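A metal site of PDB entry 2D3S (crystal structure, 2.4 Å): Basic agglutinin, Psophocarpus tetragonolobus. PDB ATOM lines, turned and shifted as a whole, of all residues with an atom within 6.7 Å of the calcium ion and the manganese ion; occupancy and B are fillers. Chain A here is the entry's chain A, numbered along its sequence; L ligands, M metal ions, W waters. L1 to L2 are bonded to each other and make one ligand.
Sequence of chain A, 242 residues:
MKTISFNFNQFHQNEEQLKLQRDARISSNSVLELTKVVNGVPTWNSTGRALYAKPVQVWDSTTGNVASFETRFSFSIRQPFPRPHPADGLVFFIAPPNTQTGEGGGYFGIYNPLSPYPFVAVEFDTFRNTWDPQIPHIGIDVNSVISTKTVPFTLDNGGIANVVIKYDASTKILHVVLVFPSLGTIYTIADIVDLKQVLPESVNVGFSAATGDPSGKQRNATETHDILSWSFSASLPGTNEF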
ATOM      1  N   ASP A  88      27.231 -10.274  11.263  1.00  0.00           N
ATOM      2  CA  ASP A  88      27.469  -8.878  11.634  1.00  0.00           C
ATOM      3  C   ASP A  88      26.554  -8.388  12.764  1.00  0.00           C
ATOM      4  O   ASP A  88      26.936  -7.531  13.565  1.00  0.00           O
ATOM      5  CB  ASP A  88      27.282  -7.961  10.414  1.00  0.00           C
ATOM      6  CG  ASP A  88      28.565  -7.786   9.633  1.00  0.00           C
ATOM      7  OD1 ASP A  88      28.786  -8.536   8.653  1.00  0.00           O
ATOM      8  OD2 ASP A  88      29.370  -6.907  10.010  1.00  0.00           O
ATOM      9  N   GLY A 105      26.705  -6.787   5.309  1.00  0.00           N
ATOM     10  CA  GLY A 105      27.827  -6.505   6.179  1.00  0.00           C
ATOM     11  C   GLY A 105      27.475  -5.566   7.324  1.00  0.00           C
ATOM     12  O   GLY A 105      26.381  -5.641   7.887  1.00  0.00           O
ATOM     13  N   GLY A 106      28.414  -4.678   7.662  1.00  0.00           N
ATOM     14  CA  GLY A 106      28.204  -3.738   8.746  1.00  0.00           C
ATOM     15  C   GLY A 106      27.022  -2.808   8.588  1.00  0.00           C
ATOM     16  O   GLY A 106      26.747  -2.001   9.480  1.00  0.00           O
ATOM     17  N   TYR A 107      26.334  -2.883   7.455  1.00  0.00           N
ATOM     18  CA  TYR A 107      25.165  -2.025   7.230  1.00  0.00           C
ATOM     19  C   TYR A 107      23.841  -2.763   7.483  1.00  0.00           C
ATOM     20  O   TYR A 107      22.759  -2.217   7.258  1.00  0.00           O
ATOM     21  CB  TYR A 107      25.197  -1.458   5.812  1.00  0.00           C
ATOM     22  CG  TYR A 107      26.353  -0.523   5.598  1.00  0.00           C
ATOM     23  CD1 TYR A 107      26.426   0.688   6.289  1.00  0.00           C
ATOM     24  CD2 TYR A 107      27.399  -0.856   4.741  1.00  0.00           C
ATOM     25  CE1 TYR A 107      27.516   1.541   6.137  1.00  0.00           C
ATOM     26  CE2 TYR A 107      28.500  -0.022   4.579  1.00  0.00           C
ATOM     27  CZ  TYR A 107      28.554   1.172   5.280  1.00  0.00           C
ATOM     28  OH  TYR A 107      29.645   1.996   5.123  1.00  0.00           O
ATOM     29  N   PHE A 108      23.963  -3.998   7.955  1.00  0.00           N
ATOM     30  CA  PHE A 108      22.830  -4.837   8.313  1.00  0.00           C
ATOM     31  C   PHE A 108      21.752  -5.043   7.257  1.00  0.00           C
ATOM     32  O   PHE A 108      20.763  -5.733   7.501  1.00  0.00           O
ATOM     33  CB  PHE A 108      22.175  -4.261   9.576  1.00  0.00           C
ATOM     34  CG  PHE A 108      23.133  -3.976  10.698  1.00  0.00           C
ATOM     35  CD1 PHE A 108      23.830  -5.011  11.312  1.00  0.00           C
ATOM     36  CD2 PHE A 108      23.291  -2.680  11.179  1.00  0.00           C
ATOM     37  CE1 PHE A 108      24.668  -4.751  12.409  1.00  0.00           C
ATOM     38  CE2 PHE A 108      24.126  -2.411  12.265  1.00  0.00           C
ATOM     39  CZ  PHE A 108      24.813  -3.455  12.883  1.00  0.00           C
ATOM     40  N   GLU A 123      20.060  -1.651  16.997  1.00  0.00           N
ATOM     41  CA  GLU A 123      20.961  -2.706  16.591  1.00  0.00           C
ATOM     42  C   GLU A 123      21.577  -3.512  17.735  1.00  0.00           C
ATOM     43  O   GLU A 123      21.750  -3.024  18.861  1.00  0.00           O
ATOM     44  CB  GLU A 123      22.111  -2.118  15.758  1.00  0.00           C
ATOM     45  CG  GLU A 123      22.921  -1.096  16.539  1.00  0.00           C
ATOM     46  CD  GLU A 123      24.185  -0.669  15.830  1.00  0.00           C
ATOM     47  OE1 GLU A 123      24.111  -0.196  14.668  1.00  0.00           O
ATOM     48  OE2 GLU A 123      25.251  -0.791  16.459  1.00  0.00           O
ATOM     49  N   ASP A 125      24.782  -5.243  17.591  1.00  0.00           N
ATOM     50  CA  ASP A 125      25.996  -5.335  16.818  1.00  0.00           C
ATOM     51  C   ASP A 125      27.061  -6.294  17.331  1.00  0.00           C
ATOM     52  O   ASP A 125      27.539  -6.159  18.454  1.00  0.00           O
ATOM     53  CB  ASP A 125      26.585  -3.942  16.717  1.00  0.00           C
ATOM     54  CG  ASP A 125      27.440  -3.769  15.503  1.00  0.00           C
ATOM     55  OD1 ASP A 125      28.112  -4.738  15.093  1.00  0.00           O
ATOM     56  OD2 ASP A 125      27.430  -2.650  14.964  1.00  0.00           O
ATOM     57  N   THR A 126      27.453  -7.256  16.500  1.00  0.00           N
ATOM     58  CA  THR A 126      28.448  -8.250  16.907  1.00  0.00           C
ATOM     59  C   THR A 126      29.830  -8.118  16.271  1.00  0.00           C
ATOM     60  O   THR A 126      30.756  -8.847  16.632  1.00  0.00           O
ATOM     61  CB  THR A 126      27.919  -9.672  16.637  1.00  0.00           C
ATOM     62  OG1 THR A 126      27.522  -9.765  15.259  1.00  0.00           O
ATOM     63  CG2 THR A 126      26.721  -9.980  17.536  1.00  0.00           C
ATOM     64  N   PHE A 127      29.979  -7.195  15.322  1.00  0.00           N
ATOM     65  CA  PHE A 127      31.260  -7.014  14.653  1.00  0.00           C
ATOM     66  C   PHE A 127      31.729  -5.563  14.725  1.00  0.00           C
ATOM     67  O   PHE A 127      30.974  -4.649  14.438  1.00  0.00           O
ATOM     68  CB  PHE A 127      31.166  -7.436  13.186  1.00  0.00           C
ATOM     69  CG  PHE A 127      32.459  -7.244  12.436  1.00  0.00           C
ATOM     70  CD1 PHE A 127      33.474  -8.200  12.515  1.00  0.00           C
ATOM     71  CD2 PHE A 127      32.680  -6.081  11.686  1.00  0.00           C
ATOM     72  CE1 PHE A 127      34.702  -7.996  11.862  1.00  0.00           C
ATOM     73  CE2 PHE A 127      33.897  -5.873  11.040  1.00  0.00           C
ATOM     74  CZ  PHE A 127      34.914  -6.823  11.132  1.00  0.00           C
ATOM     75  N   ARG A 128      32.989  -5.350  15.081  1.00  0.00           N
ATOM     76  CA  ARG A 128      33.478  -3.989  15.175  1.00  0.00           C
ATOM     77  C   ARG A 128      33.931  -3.368  13.854  1.00  0.00           C
ATOM     78  O   ARG A 128      35.008  -3.668  13.353  1.00  0.00           O
ATOM     79  CB  ARG A 128      34.621  -3.914  16.184  1.00  0.00           C
ATOM     80  CG  ARG A 128      34.935  -2.492  16.595  1.00  0.00           C
ATOM     81  CD  ARG A 128      35.870  -2.460  17.782  1.00  0.00           C
ATOM     82  NE  ARG A 128      36.010  -1.095  18.270  1.00  0.00           N
ATOM     83  CZ  ARG A 128      36.803  -0.741  19.280  1.00  0.00           C
ATOM     84  NH1 ARG A 128      37.531  -1.654  19.913  1.00  0.00           N
ATOM     85  NH2 ARG A 128      36.860   0.532  19.655  1.00  0.00           N
ATOM     86  N   ASN A 129      33.092  -2.525  13.279  1.00  0.00           N
ATOM     87  CA  ASN A 129      33.435  -1.840  12.036  1.00  0.00           C
ATOM     88  C   ASN A 129      34.289  -0.641  12.420  1.00  0.00           C
ATOM     89  O   ASN A 129      34.379  -0.308  13.608  1.00  0.00           O
ATOM     90  CB  ASN A 129      32.167  -1.410  11.312  1.00  0.00           C
ATOM     91  CG  ASN A 129      31.625  -2.479  10.392  1.00  0.00           C
ATOM     92  OD1 ASN A 129      32.007  -2.570   9.210  1.00  0.00           O
ATOM     93  ND2 ASN A 129      30.744  -3.319  10.917  1.00  0.00           N
ATOM     94  N   TRP A 131      33.738   2.293  12.443  1.00  0.00           N
ATOM     95  CA  TRP A 131      32.914   3.250  13.185  1.00  0.00           C
ATOM     96  C   TRP A 131      32.272   2.749  14.484  1.00  0.00           C
ATOM     97  O   TRP A 131      31.412   3.442  15.015  1.00  0.00           O
ATOM     98  CB  TRP A 131      31.798   3.750  12.275  1.00  0.00           C
ATOM     99  CG  TRP A 131      30.851   2.659  11.898  1.00  0.00           C
ATOM    100  CD1 TRP A 131      29.897   2.086  12.687  1.00  0.00           C
ATOM    101  CD2 TRP A 131      30.799   1.966  10.644  1.00  0.00           C
ATOM    102  NE1 TRP A 131      29.262   1.076  12.019  1.00  0.00           N
ATOM    103  CE2 TRP A 131      29.794   0.976  10.756  1.00  0.00           C
ATOM    104  CE3 TRP A 131      31.509   2.069   9.439  1.00  0.00           C
ATOM    105  CZ2 TRP A 131      29.478   0.106   9.713  1.00  0.00           C
ATOM    106  CZ3 TRP A 131      31.186   1.207   8.395  1.00  0.00           C
ATOM    107  CH2 TRP A 131      30.175   0.231   8.541  1.00  0.00           C
ATOM    108  N   ASP A 132      32.660   1.585  14.988  1.00  0.00           N
ATOM    109  CA  ASP A 132      32.053   1.078  16.223  1.00  0.00           C
ATOM    110  C   ASP A 132      32.943   1.054  17.422  1.00  0.00           C
ATOM    111  O   ASP A 132      34.170   1.054  17.313  1.00  0.00           O
ATOM    112  CB  ASP A 132      31.578  -0.375  16.092  1.00  0.00           C
ATOM    113  CG  ASP A 132      30.550  -0.575  15.026  1.00  0.00           C
ATOM    114  OD1 ASP A 132      29.565   0.173  14.979  1.00  0.00           O
ATOM    115  OD2 ASP A 132      30.747  -1.510  14.238  1.00  0.00           O
ATOM    116  N   PRO A 133      32.322   1.024  18.616  1.00  0.00           N
ATOM    117  CA  PRO A 133      33.024   0.957  19.891  1.00  0.00           C
ATOM    118  C   PRO A 133      33.092  -0.556  20.106  1.00  0.00           C
ATOM    119  O   PRO A 133      32.684  -1.327  19.225  1.00  0.00           O
ATOM    120  CB  PRO A 133      32.061   1.636  20.853  1.00  0.00           C
ATOM    121  CG  PRO A 133      30.736   1.246  20.305  1.00  0.00           C
ATOM    122  CD  PRO A 133      30.923   1.455  18.817  1.00  0.00           C
ATOM    123  N   ILE A 135      32.497  -4.353  20.665  1.00  0.00           N
ATOM    124  CA  ILE A 135      31.319  -5.187  20.436  1.00  0.00           C
ATOM    125  C   ILE A 135      31.364  -6.350  21.426  1.00  0.00           C
ATOM    126  O   ILE A 135      32.422  -6.670  21.960  1.00  0.00           O
ATOM    127  CB  ILE A 135      31.265  -5.713  18.962  1.00  0.00           C
ATOM    128  CG1 ILE A 135      32.601  -6.362  18.561  1.00  0.00           C
ATOM    129  CG2 ILE A 135      30.913  -4.574  18.022  1.00  0.00           C
ATOM    130  CD1 ILE A 135      32.833  -7.767  19.131  1.00  0.00           C
ATOM    131  N   HIS A 137      27.401  -4.718  21.215  1.00  0.00           N
ATOM    132  CA  HIS A 137      26.773  -3.574  21.851  1.00  0.00           C
ATOM    133  C   HIS A 137      25.402  -3.321  21.253  1.00  0.00           C
ATOM    134  O   HIS A 137      25.123  -3.715  20.124  1.00  0.00           O
ATOM    135  CB  HIS A 137      27.633  -2.317  21.726  1.00  0.00           C
ATOM    136  CG  HIS A 137      27.938  -1.918  20.311  1.00  0.00           C
ATOM    137  ND1 HIS A 137      29.169  -2.155  19.725  1.00  0.00           N
ATOM    138  CD2 HIS A 137      27.187  -1.306  19.365  1.00  0.00           C
ATOM    139  CE1 HIS A 137      29.153  -1.698  18.484  1.00  0.00           C
ATOM    140  NE2 HIS A 137      27.958  -1.184  18.235  1.00  0.00           N
ATOM    141  N   ILE A 138      24.551  -2.679  22.044  1.00  0.00           N
ATOM    142  CA  ILE A 138      23.217  -2.298  21.614  1.00  0.00           C
ATOM    143  C   ILE A 138      23.401  -0.870  21.154  1.00  0.00           C
ATOM    144  O   ILE A 138      24.202  -0.126  21.732  1.00  0.00           O
ATOM    145  CB  ILE A 138      22.225  -2.276  22.780  1.00  0.00           C
ATOM    146  CG1 ILE A 138      22.267  -3.604  23.540  1.00  0.00           C
ATOM    147  CG2 ILE A 138      20.841  -1.994  22.249  1.00  0.00           C
ATOM    148  CD1 ILE A 138      21.453  -3.593  24.827  1.00  0.00           C
ATOM    149  N   GLY A 139      22.693  -0.476  20.119  1.00  0.00           N
ATOM    150  CA  GLY A 139      22.854   0.886  19.656  1.00  0.00           C
ATOM    151  C   GLY A 139      21.578   1.438  19.080  1.00  0.00           C
ATOM    152  O   GLY A 139      20.759   0.695  18.526  1.00  0.00           O
ATOM    153  N   ASP A 141      20.192   3.795  16.304  1.00  0.00           N
ATOM    154  CA  ASP A 141      20.595   4.361  15.027  1.00  0.00           C
ATOM    155  C   ASP A 141      19.532   5.223  14.381  1.00  0.00           C
ATOM    156  O   ASP A 141      18.384   4.809  14.239  1.00  0.00           O
ATOM    157  CB  ASP A 141      20.981   3.247  14.046  1.00  0.00           C
ATOM    158  CG  ASP A 141      22.045   2.334  14.581  1.00  0.00           C
ATOM    159  OD1 ASP A 141      22.693   2.700  15.585  1.00  0.00           O
ATOM    160  OD2 ASP A 141      22.254   1.242  14.007  1.00  0.00           O
ATOM    161  N   VAL A 145      24.287   4.137  10.623  1.00  0.00           N
ATOM    162  CA  VAL A 145      24.697   2.979  11.395  1.00  0.00           C
ATOM    163  C   VAL A 145      25.701   3.438  12.454  1.00  0.00           C
ATOM    164  O   VAL A 145      26.205   2.650  13.252  1.00  0.00           O
ATOM    165  CB  VAL A 145      25.314   1.906  10.469  1.00  0.00           C
ATOM    166  CG1 VAL A 145      26.182   0.946  11.241  1.00  0.00           C
ATOM    167  CG2 VAL A 145      24.188   1.132   9.785  1.00  0.00           C
ATOM    168  N   ILE A 146      25.994   4.740  12.448  1.00  0.00           N
ATOM    169  CA  ILE A 146      26.890   5.307  13.441  1.00  0.00           C
ATOM    170  C   ILE A 146      25.930   5.733  14.547  1.00  0.00           C
ATOM    171  O   ILE A 146      25.353   6.819  14.511  1.00  0.00           O
ATOM    172  CB  ILE A 146      27.647   6.525  12.860  1.00  0.00           C
ATOM    173  CG1 ILE A 146      28.552   6.051  11.719  1.00  0.00           C
ATOM    174  CG2 ILE A 146      28.454   7.224  13.955  1.00  0.00           C
ATOM    175  CD1 ILE A 146      29.204   7.165  10.934  1.00  0.00           C
ATOM    176  N   SER A 147      25.761   4.836  15.504  1.00  0.00           N
ATOM    177  CA  SER A 147      24.837   5.016  16.625  1.00  0.00           C
ATOM    178  C   SER A 147      24.966   6.315  17.406  1.00  0.00           C
ATOM    179  O   SER A 147      26.063   6.793  17.684  1.00  0.00           O
ATOM    180  CB  SER A 147      24.981   3.848  17.601  1.00  0.00           C
ATOM    181  OG  SER A 147      24.858   2.617  16.917  1.00  0.00           O
ATOM    182  N   THR A 150      25.245   4.146  22.574  1.00  0.00           N
ATOM    183  CA  THR A 150      25.670   2.759  22.574  1.00  0.00           C
ATOM    184  C   THR A 150      25.898   2.191  23.982  1.00  0.00           C
ATOM    185  O   THR A 150      26.265   2.915  24.902  1.00  0.00           O
ATOM    186  CB  THR A 150      26.992   2.607  21.745  1.00  0.00           C
ATOM    187  OG1 THR A 150      26.678   2.411  20.368  1.00  0.00           O
ATOM    188  CG2 THR A 150      27.831   1.462  22.239  1.00  0.00           C
HETATM  189  N1  LIG L   1      37.479  -5.687   7.988  1.00  0.00           N
HETATM  190  C1  LIG L   1      37.003  -4.849   6.879  1.00  0.00           C
HETATM  191  C2  LIG L   1      36.361  -3.544   7.390  1.00  0.00           C
HETATM  192  O1  LIG L   1      35.845  -2.737   6.602  1.00  0.00           O
HETATM  193  C3  LIG L   1      36.009  -5.668   6.031  1.00  0.00           C
HETATM  194  O2  LIG L   1      34.818  -5.920   6.756  1.00  0.00           O
HETATM  195  O3  LIG L   1      36.352  -3.275   8.609  1.00  0.00           O
HETATM  196  O1  LG2 L   2      33.686  -7.928   6.343  1.00  0.00           O
HETATM  197  C1  LG2 L   2      33.697  -6.502   6.086  1.00  0.00           C
HETATM  198  C2  LG2 L   2      32.414  -5.846   6.612  1.00  0.00           C
HETATM  199  N1  LG2 L   2      32.496  -4.422   6.352  1.00  0.00           N
HETATM  200  C3  LG2 L   2      32.264  -6.143   8.118  1.00  0.00           C
HETATM  201  O2  LG2 L   2      31.076  -5.539   8.619  1.00  0.00           O
HETATM  202  C4  LG2 L   2      32.218  -7.655   8.329  1.00  0.00           C
HETATM  203  O3  LG2 L   2      31.081  -8.171   7.645  1.00  0.00           O
HETATM  204  C5  LG2 L   2      33.509  -8.258   7.751  1.00  0.00           C
HETATM  205  C6  LG2 L   2      33.517  -9.770   7.908  1.00  0.00           C
HETATM  206  O4  LG2 L   2      34.831 -10.240   7.583  1.00  0.00           O
HETATM  207  C7  LG2 L   2      31.564  -3.751   5.663  1.00  0.00           C
HETATM  208  O5  LG2 L   2      30.568  -4.304   5.221  1.00  0.00           O
HETATM  209  C8  LG2 L   2      31.817  -2.281   5.489  1.00  0.00           C
HETATM  210 CA    CA M   1      29.289  -3.293  13.164  1.00  0.00          CA
HETATM  211 MN    MN M   2      27.575  -0.570  15.999  1.00  0.00          MN
HETATM  212  O   HOH W   1      27.244   1.605  16.536  1.00  0.00           O
HETATM  213  O   HOH W   2      28.023  -5.258  11.731  1.00  0.00           O
HETATM  214  O   HOH W   3      27.489  -1.783  12.021  1.00  0.00           O
HETATM  215  O   HOH W   4      26.859   0.086  14.051  1.00  0.00           O
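The side-chain amide oxygen (OD1) of Asn 129 sits at hydrogen-bond distance from an oxygen (O2) of LG2 L2 (3.2 Å). An oxygen (O2) of LG2 L2 lies within hydrogen-bond range of the backbone NH of Gly 106 (3.0 Å). An oxygen (O3) of LG2 L2 lies within hydrogen-bond range of the side-chain carboxylate of Asp 88.
The indole nitrogen of Trp 131 sits close to the side-chain carboxylate of Asp 132, 3.1 Å away. NE of Arg 128 is in hydrogen-bond range of O of Asp 132, at 3.0 Å. The side-chain carboxylate (OE2) of Glu 123 lies close to the side-chain hydroxyl (OG) of Ser 147 (3.5 Å). The side-chain carboxylate of Glu 123 lies close to the side-chain carboxylate of Asp 141. The backbone carbonyl oxygen (O) of Gly 139 is in hydrogen-bond range of the backbone NH (N) of Glu 123.
Four residues have an atom within 4 Å of the calcium ion: Asp 125, Phe 127, Asn 129 and Asp 132. The nearest printed residue that does not touch the calcium ion is Phe 108 (4.5 Å).
The calcium ion is bound by O of Phe 127 (2.5 Å), OD2 of Asp 132 (2.5 Å), water W3 (2.6 Å), OD2 of Asp 125 (2.7 Å), ND2 of Asn 129 (2.7 Å), OD1 of Asp 125 (2.7 Å) and water W2 (2.7 Å).
The manganese ion is bound by water W4 (2.2 Å), water W1 (2.3 Å), OD2 of Asp 125 (2.3 Å), NE2 of His 137 (2.4 Å), OD1 of Asp 132 (2.4 Å) and OE2 of Glu 123 (2.4 Å).
Water W3 lies within hydrogen-bond range of the backbone carbonyl oxygen (O) of Gly 106 (2.7 Å) and the indole nitrogen (NE1) of Trp 131 (3.4 Å). Water W4 lies within hydrogen-bond range of O of Val 145 (2.8 Å), OE1 of Glu 123 (2.8 Å) and NE1 of Trp 131 (3.3 Å).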
